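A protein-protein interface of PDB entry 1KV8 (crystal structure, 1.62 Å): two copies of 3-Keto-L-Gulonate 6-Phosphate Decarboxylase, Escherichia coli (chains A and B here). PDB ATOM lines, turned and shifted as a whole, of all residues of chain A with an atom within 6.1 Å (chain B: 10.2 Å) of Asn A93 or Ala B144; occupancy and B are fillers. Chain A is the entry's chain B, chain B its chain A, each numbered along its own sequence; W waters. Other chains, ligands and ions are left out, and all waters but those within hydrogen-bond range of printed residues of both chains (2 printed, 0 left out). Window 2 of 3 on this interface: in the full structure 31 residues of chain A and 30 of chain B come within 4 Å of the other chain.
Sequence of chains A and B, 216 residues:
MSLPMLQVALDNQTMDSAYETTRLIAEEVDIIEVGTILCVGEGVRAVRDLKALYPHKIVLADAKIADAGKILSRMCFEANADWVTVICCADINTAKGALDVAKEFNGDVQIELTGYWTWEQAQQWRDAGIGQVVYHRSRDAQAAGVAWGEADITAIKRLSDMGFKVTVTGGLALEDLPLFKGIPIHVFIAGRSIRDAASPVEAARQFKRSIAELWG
The backbone NH (N) of Gly A69 is in hydrogen-bond range of the side-chain carboxylate (OD2) of Asp B140 (2.9 Å).
OD2 of Asp B140 is in hydrogen-bond range of OG1 of Thr A94 (2.7 Å).
Of chain B, only Asp B140 (3.8 Å) and Ala B144 (3.3 Å) come within 4 Å of Asn A93.
Ala B144 touches just one residue of chain A: Asn A93.
Asp A91 touches just these residues of chain B: Ser B138 and Ala B141.
Of the printed residues of chain B, Thr A94 touches Asp B140 (2.7 Å).
No residue of chain B comes within 4 Å of Ala A95.
Lys A96 touches none of the printed residues of chain B.
Printed residues of chain A within 4 Å of Ala B141: Asp A91.
Of the printed residues of chain B, Gly A69 touches Asp B140.
Printed residues of chain A within 4 Å of Ser B138: Asp A91.
Arg B139 touches none of the printed residues of chain A.
Arg B137 touches none of the printed residues of chain A.
The nearest residue of chain B that does not touch Asn A93 is Ala B141 (4.3 Å).
The nearest residue of chain A that does not touch Ala B144 is Asp A91 (5.5 Å).
The nearest printed residue of chain A that does not touch Ser B138 is Thr A94 (4.3 Å).
Water W2 bridges OD1 of Asp B140 (2.6 Å) and N of Gly A69 (3.4 Å).
Water W1 lies within hydrogen-bond range of the side-chain hydroxyl (OG1) of Thr A94 (2.6 Å), the backbone NH (N) of Asp A91 (2.8 Å) and the side-chain hydroxyl (OG) of Ser B138 (3.2 Å).
No position is printed for both chains.
Among the printed residues, merely in contact across the chains: Asp A91 with Ser B138 (3.9 Å), Asp A91 with Ala B141 (3.9 Å), Asn A93 with Asp B140 (3.8 Å) and Asn A93 with Ala B144 (3.3 Å).
Along chain B the printed residues that touch a printed residue of chain A span positions 138 to 144.
N of Ala B141 is in hydrogen-bond range of OG of Ser B138, at 3.2 Å.
N of Val B146 sits at hydrogen-bond distance from O of Ala B141, at 3.0 Å.
OG1 of Thr A94 lies close to O of Asp A91 (3.4 Å).
The side-chain carboxylate (OD2) of Asp A91 is in hydrogen-bond range of the side-chain amide nitrogen (ND2) of Asn A93 (2.7 Å).
The backbone NH (N) of Asp B140 lies within hydrogen-bond range of the side-chain hydroxyl (OG) of Ser B138 (3.2 Å).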
ATOM      1  N   GLY A  69      12.242  -3.870  -1.379  1.00  0.00           N
ATOM      2  CA  GLY A  69      13.534  -4.079  -0.746  1.00  0.00           C
ATOM      3  C   GLY A  69      14.728  -4.038  -1.681  1.00  0.00           C
ATOM      4  O   GLY A  69      15.749  -3.427  -1.365  1.00  0.00           O
ATOM      5  N   ALA A  90       7.691  -4.959   7.559  1.00  0.00           N
ATOM      6  CA  ALA A  90       7.863  -5.339   6.159  1.00  0.00           C
ATOM      7  C   ALA A  90       7.710  -6.835   5.901  1.00  0.00           C
ATOM      8  O   ALA A  90       8.050  -7.664   6.747  1.00  0.00           O
ATOM      9  CB  ALA A  90       9.225  -4.870   5.659  1.00  0.00           C
ATOM     10  N   ASP A  91       7.189  -7.171   4.725  1.00  0.00           N
ATOM     11  CA  ASP A  91       7.024  -8.565   4.336  1.00  0.00           C
ATOM     12  C   ASP A  91       8.420  -9.176   4.402  1.00  0.00           C
ATOM     13  O   ASP A  91       9.406  -8.525   4.040  1.00  0.00           O
ATOM     14  CB  ASP A  91       6.485  -8.654   2.903  1.00  0.00           C
ATOM     15  CG  ASP A  91       6.194 -10.081   2.473  1.00  0.00           C
ATOM     16  OD1 ASP A  91       5.120 -10.607   2.836  1.00  0.00           O
ATOM     17  OD2 ASP A  91       7.044 -10.680   1.779  1.00  0.00           O
ATOM     18  N   ILE A  92       8.515 -10.420   4.858  1.00  0.00           N
ATOM     19  CA  ILE A  92       9.812 -11.068   4.971  1.00  0.00           C
ATOM     20  C   ILE A  92      10.602 -11.026   3.663  1.00  0.00           C
ATOM     21  O   ILE A  92      11.830 -10.983   3.678  1.00  0.00           O
ATOM     22  CB  ILE A  92       9.671 -12.535   5.445  1.00  0.00           C
ATOM     23  CG1 ILE A  92      11.048 -13.104   5.784  1.00  0.00           C
ATOM     24  CG2 ILE A  92       8.990 -13.375   4.374  1.00  0.00           C
ATOM     25  CD1 ILE A  92      11.760 -12.350   6.900  1.00  0.00           C
ATOM     26  N   ASN A  93       9.902 -11.027   2.533  1.00  0.00           N
ATOM     27  CA  ASN A  93      10.580 -10.985   1.243  1.00  0.00           C
ATOM     28  C   ASN A  93      11.282  -9.653   1.003  1.00  0.00           C
ATOM     29  O   ASN A  93      12.200  -9.561   0.187  1.00  0.00           O
ATOM     30  CB  ASN A  93       9.585 -11.271   0.122  1.00  0.00           C
ATOM     31  CG  ASN A  93       9.093 -12.698   0.149  1.00  0.00           C
ATOM     32  OD1 ASN A  93       9.876 -13.635  -0.013  1.00  0.00           O
ATOM     33  ND2 ASN A  93       7.797 -12.878   0.367  1.00  0.00           N
ATOM     34  N   THR A  94      10.852  -8.625   1.726  1.00  0.00           N
ATOM     35  CA  THR A  94      11.460  -7.306   1.608  1.00  0.00           C
ATOM     36  C   THR A  94      12.830  -7.362   2.281  1.00  0.00           C
ATOM     37  O   THR A  94      13.821  -6.886   1.731  1.00  0.00           O
ATOM     38  CB  THR A  94      10.590  -6.224   2.295  1.00  0.00           C
ATOM     39  OG1 THR A  94       9.329  -6.124   1.620  1.00  0.00           O
ATOM     40  CG2 THR A  94      11.285  -4.870   2.259  1.00  0.00           C
ATOM     41  N   ALA A  95      12.883  -7.956   3.471  1.00  0.00           N
ATOM     42  CA  ALA A  95      14.145  -8.077   4.190  1.00  0.00           C
ATOM     43  C   ALA A  95      15.101  -8.935   3.369  1.00  0.00           C
ATOM     44  O   ALA A  95      16.280  -8.614   3.238  1.00  0.00           O
ATOM     45  CB  ALA A  95      13.919  -8.709   5.564  1.00  0.00           C
ATOM     46  N   LYS A  96      14.587 -10.028   2.812  1.00  0.00           N
ATOM     47  CA  LYS A  96      15.410 -10.916   2.001  1.00  0.00           C
ATOM     48  C   LYS A  96      15.947 -10.199   0.767  1.00  0.00           C
ATOM     49  O   LYS A  96      17.104 -10.373   0.393  1.00  0.00           O
ATOM     50  CB  LYS A  96      14.608 -12.148   1.570  1.00  0.00           C
ATOM     51  CG  LYS A  96      14.310 -13.126   2.695  1.00  0.00           C
ATOM     52  CD  LYS A  96      13.606 -14.365   2.164  1.00  0.00           C
ATOM     53  CE  LYS A  96      13.331 -15.369   3.270  1.00  0.00           C
ATOM     54  NZ  LYS A  96      12.635 -16.584   2.748  1.00  0.00           N
ATOM     55  N   GLY A  97      15.097  -9.393   0.136  1.00  0.00           N
ATOM     56  CA  GLY A  97      15.516  -8.665  -1.049  1.00  0.00           C
ATOM     57  C   GLY A  97      16.612  -7.664  -0.737  1.00  0.00           C
ATOM     58  O   GLY A  97      17.593  -7.548  -1.476  1.00  0.00           O
ATOM     59  N   ALA A  98      16.442  -6.932   0.360  1.00  0.00           N
ATOM     60  CA  ALA A  98      17.427  -5.941   0.765  1.00  0.00           C
ATOM     61  C   ALA A  98      18.746  -6.619   1.112  1.00  0.00           C
ATOM     62  O   ALA A  98      19.817  -6.119   0.776  1.00  0.00           O
ATOM     63  CB  ALA A  98      16.913  -5.154   1.966  1.00  0.00           C
ATOM     64  N   THR B 114       1.077  -1.781   4.329  1.00  0.00           N
ATOM     65  CA  THR B 114       2.080  -2.573   3.636  1.00  0.00           C
ATOM     66  C   THR B 114       2.786  -3.353   4.727  1.00  0.00           C
ATOM     67  O   THR B 114       3.390  -2.770   5.627  1.00  0.00           O
ATOM     68  CB  THR B 114       3.107  -1.687   2.907  1.00  0.00           C
ATOM     69  OG1 THR B 114       2.499  -1.119   1.739  1.00  0.00           O
ATOM     70  CG2 THR B 114       4.330  -2.505   2.495  1.00  0.00           C
ATOM     71  N   GLY B 115       2.700  -4.674   4.650  1.00  0.00           N
ATOM     72  CA  GLY B 115       3.333  -5.494   5.661  1.00  0.00           C
ATOM     73  C   GLY B 115       2.332  -5.960   6.699  1.00  0.00           C
ATOM     74  O   GLY B 115       1.126  -5.997   6.448  1.00  0.00           O
ATOM     75  N   TYR B 116       2.832  -6.294   7.880  1.00  0.00           N
ATOM     76  CA  TYR B 116       1.996  -6.799   8.961  1.00  0.00           C
ATOM     77  C   TYR B 116       1.359  -5.757   9.877  1.00  0.00           C
ATOM     78  O   TYR B 116       2.016  -4.819  10.321  1.00  0.00           O
ATOM     79  CB  TYR B 116       2.823  -7.774   9.805  1.00  0.00           C
ATOM     80  CG  TYR B 116       2.146  -8.230  11.076  1.00  0.00           C
ATOM     81  CD1 TYR B 116       0.982  -8.995  11.037  1.00  0.00           C
ATOM     82  CD2 TYR B 116       2.677  -7.901  12.324  1.00  0.00           C
ATOM     83  CE1 TYR B 116       0.363  -9.425  12.209  1.00  0.00           C
ATOM     84  CE2 TYR B 116       2.067  -8.324  13.500  1.00  0.00           C
ATOM     85  CZ  TYR B 116       0.913  -9.085  13.436  1.00  0.00           C
ATOM     86  OH  TYR B 116       0.313  -9.512  14.596  1.00  0.00           O
ATOM     87  N   ARG B 137      -1.096  -4.670  -1.428  1.00  0.00           N
ATOM     88  CA  ARG B 137      -0.462  -5.975  -1.570  1.00  0.00           C
ATOM     89  C   ARG B 137       0.995  -5.630  -1.853  1.00  0.00           C
ATOM     90  O   ARG B 137       1.305  -5.010  -2.870  1.00  0.00           O
ATOM     91  CB  ARG B 137      -1.036  -6.768  -2.751  1.00  0.00           C
ATOM     92  CG  ARG B 137      -0.323  -8.100  -2.959  1.00  0.00           C
ATOM     93  CD  ARG B 137      -0.829  -8.867  -4.180  1.00  0.00           C
ATOM     94  NE  ARG B 137      -0.636  -8.129  -5.426  1.00  0.00           N
ATOM     95  CZ  ARG B 137      -0.627  -8.691  -6.632  1.00  0.00           C
ATOM     96  NH1 ARG B 137      -0.789 -10.002  -6.760  1.00  0.00           N
ATOM     97  NH2 ARG B 137      -0.474  -7.942  -7.716  1.00  0.00           N
ATOM     98  N   SER B 138       1.879  -6.013  -0.940  1.00  0.00           N
ATOM     99  CA  SER B 138       3.304  -5.734  -1.071  1.00  0.00           C
ATOM    100  C   SER B 138       3.882  -6.107  -2.436  1.00  0.00           C
ATOM    101  O   SER B 138       3.570  -7.163  -2.988  1.00  0.00           O
ATOM    102  CB  SER B 138       4.071  -6.478   0.029  1.00  0.00           C
ATOM    103  OG  SER B 138       5.467  -6.475  -0.209  1.00  0.00           O
ATOM    104  N   ARG B 139       4.727  -5.231  -2.972  1.00  0.00           N
ATOM    105  CA  ARG B 139       5.384  -5.468  -4.255  1.00  0.00           C
ATOM    106  C   ARG B 139       6.268  -6.704  -4.123  1.00  0.00           C
ATOM    107  O   ARG B 139       6.345  -7.531  -5.031  1.00  0.00           O
ATOM    108  CB  ARG B 139       6.246  -4.258  -4.631  1.00  0.00           C
ATOM    109  CG  ARG B 139       7.158  -4.461  -5.832  1.00  0.00           C
ATOM    110  CD  ARG B 139       8.217  -3.363  -5.890  1.00  0.00           C
ATOM    111  NE  ARG B 139       7.632  -2.037  -6.076  1.00  0.00           N
ATOM    112  CZ  ARG B 139       7.532  -1.417  -7.248  1.00  0.00           C
ATOM    113  NH1 ARG B 139       7.986  -1.998  -8.352  1.00  0.00           N
ATOM    114  NH2 ARG B 139       6.971  -0.216  -7.317  1.00  0.00           N
ATOM    115  N   ASP B 140       6.932  -6.828  -2.979  1.00  0.00           N
ATOM    116  CA  ASP B 140       7.809  -7.965  -2.745  1.00  0.00           C
ATOM    117  C   ASP B 140       7.023  -9.248  -2.511  1.00  0.00           C
ATOM    118  O   ASP B 140       7.479 -10.332  -2.873  1.00  0.00           O
ATOM    119  CB  ASP B 140       8.747  -7.676  -1.573  1.00  0.00           C
ATOM    120  CG  ASP B 140       9.723  -6.556  -1.882  1.00  0.00           C
ATOM    121  OD1 ASP B 140      10.037  -6.360  -3.076  1.00  0.00           O
ATOM    122  OD2 ASP B 140      10.189  -5.883  -0.943  1.00  0.00           O
ATOM    123  N   ALA B 141       5.844  -9.130  -1.908  1.00  0.00           N
ATOM    124  CA  ALA B 141       5.005 -10.298  -1.674  1.00  0.00           C
ATOM    125  C   ALA B 141       4.517 -10.760  -3.046  1.00  0.00           C
ATOM    126  O   ALA B 141       4.512 -11.954  -3.355  1.00  0.00           O
ATOM    127  CB  ALA B 141       3.821  -9.930  -0.790  1.00  0.00           C
ATOM    128  N   GLN B 142       4.112  -9.793  -3.864  1.00  0.00           N
ATOM    129  CA  GLN B 142       3.632 -10.062  -5.218  1.00  0.00           C
ATOM    130  C   GLN B 142       4.706 -10.801  -6.007  1.00  0.00           C
ATOM    131  O   GLN B 142       4.423 -11.777  -6.704  1.00  0.00           O
ATOM    132  CB  GLN B 142       3.299  -8.742  -5.924  1.00  0.00           C
ATOM    133  CG  GLN B 142       2.938  -8.884  -7.400  1.00  0.00           C
ATOM    134  CD  GLN B 142       2.858  -7.545  -8.112  1.00  0.00           C
ATOM    135  OE1 GLN B 142       2.910  -6.489  -7.480  1.00  0.00           O
ATOM    136  NE2 GLN B 142       2.727  -7.584  -9.434  1.00  0.00           N
ATOM    137  N   ALA B 143       5.940 -10.325  -5.898  1.00  0.00           N
ATOM    138  CA  ALA B 143       7.055 -10.939  -6.607  1.00  0.00           C
ATOM    139  C   ALA B 143       7.311 -12.351  -6.095  1.00  0.00           C
ATOM    140  O   ALA B 143       7.888 -13.180  -6.803  1.00  0.00           O
ATOM    141  CB  ALA B 143       8.307 -10.087  -6.447  1.00  0.00           C
ATOM    142  N   ALA B 144       6.878 -12.622  -4.865  1.00  0.00           N
ATOM    143  CA  ALA B 144       7.060 -13.937  -4.256  1.00  0.00           C
ATOM    144  C   ALA B 144       5.905 -14.885  -4.573  1.00  0.00           C
ATOM    145  O   ALA B 144       5.838 -15.992  -4.033  1.00  0.00           O
ATOM    146  CB  ALA B 144       7.225 -13.798  -2.749  1.00  0.00           C
ATOM    147  N   GLY B 145       4.992 -14.446  -5.436  1.00  0.00           N
ATOM    148  CA  GLY B 145       3.871 -15.289  -5.818  1.00  0.00           C
ATOM    149  C   GLY B 145       2.549 -15.042  -5.114  1.00  0.00           C
ATOM    150  O   GLY B 145       1.572 -15.745  -5.371  1.00  0.00           O
ATOM    151  N   VAL B 146       2.503 -14.054  -4.228  1.00  0.00           N
ATOM    152  CA  VAL B 146       1.270 -13.755  -3.510  1.00  0.00           C
ATOM    153  C   VAL B 146       0.285 -13.024  -4.415  1.00  0.00           C
ATOM    154  O   VAL B 146       0.547 -11.909  -4.866  1.00  0.00           O
ATOM    155  CB  VAL B 146       1.543 -12.891  -2.266  1.00  0.00           C
ATOM    156  CG1 VAL B 146       0.239 -12.598  -1.540  1.00  0.00           C
ATOM    157  CG2 VAL B 146       2.515 -13.608  -1.346  1.00  0.00           C
ATOM    158  N   ALA B 147      -0.851 -13.660  -4.681  1.00  0.00           N
ATOM    159  CA  ALA B 147      -1.869 -13.067  -5.536  1.00  0.00           C
ATOM    160  C   ALA B 147      -3.018 -12.512  -4.709  1.00  0.00           C
ATOM    161  O   ALA B 147      -3.111 -12.769  -3.509  1.00  0.00           O
ATOM    162  CB  ALA B 147      -2.392 -14.110  -6.518  1.00  0.00           C
ATOM    163  N   ARG B 192       3.003   0.642 -12.024  1.00  0.00           N
ATOM    164  CA  ARG B 192       3.568  -0.052 -13.173  1.00  0.00           C
ATOM    165  C   ARG B 192       2.608  -0.245 -14.350  1.00  0.00           C
ATOM    166  O   ARG B 192       3.010  -0.093 -15.504  1.00  0.00           O
ATOM    167  CB  ARG B 192       4.122  -1.410 -12.728  1.00  0.00           C
ATOM    168  CG  ARG B 192       5.436  -1.317 -11.959  1.00  0.00           C
ATOM    169  CD  ARG B 192       5.738  -2.605 -11.210  1.00  0.00           C
ATOM    170  NE  ARG B 192       4.863  -2.761 -10.051  1.00  0.00           N
ATOM    171  CZ  ARG B 192       4.791  -3.859  -9.305  1.00  0.00           C
ATOM    172  NH1 ARG B 192       3.966  -3.901  -8.268  1.00  0.00           N
ATOM    173  NH2 ARG B 192       5.536  -4.917  -9.601  1.00  0.00           N
HETATM  174  O   HOH W   1       6.928  -5.490   2.509  1.00  0.00           O
HETATM  175  O   HOH W   2      12.564  -6.487  -3.543  1.00  0.00           O
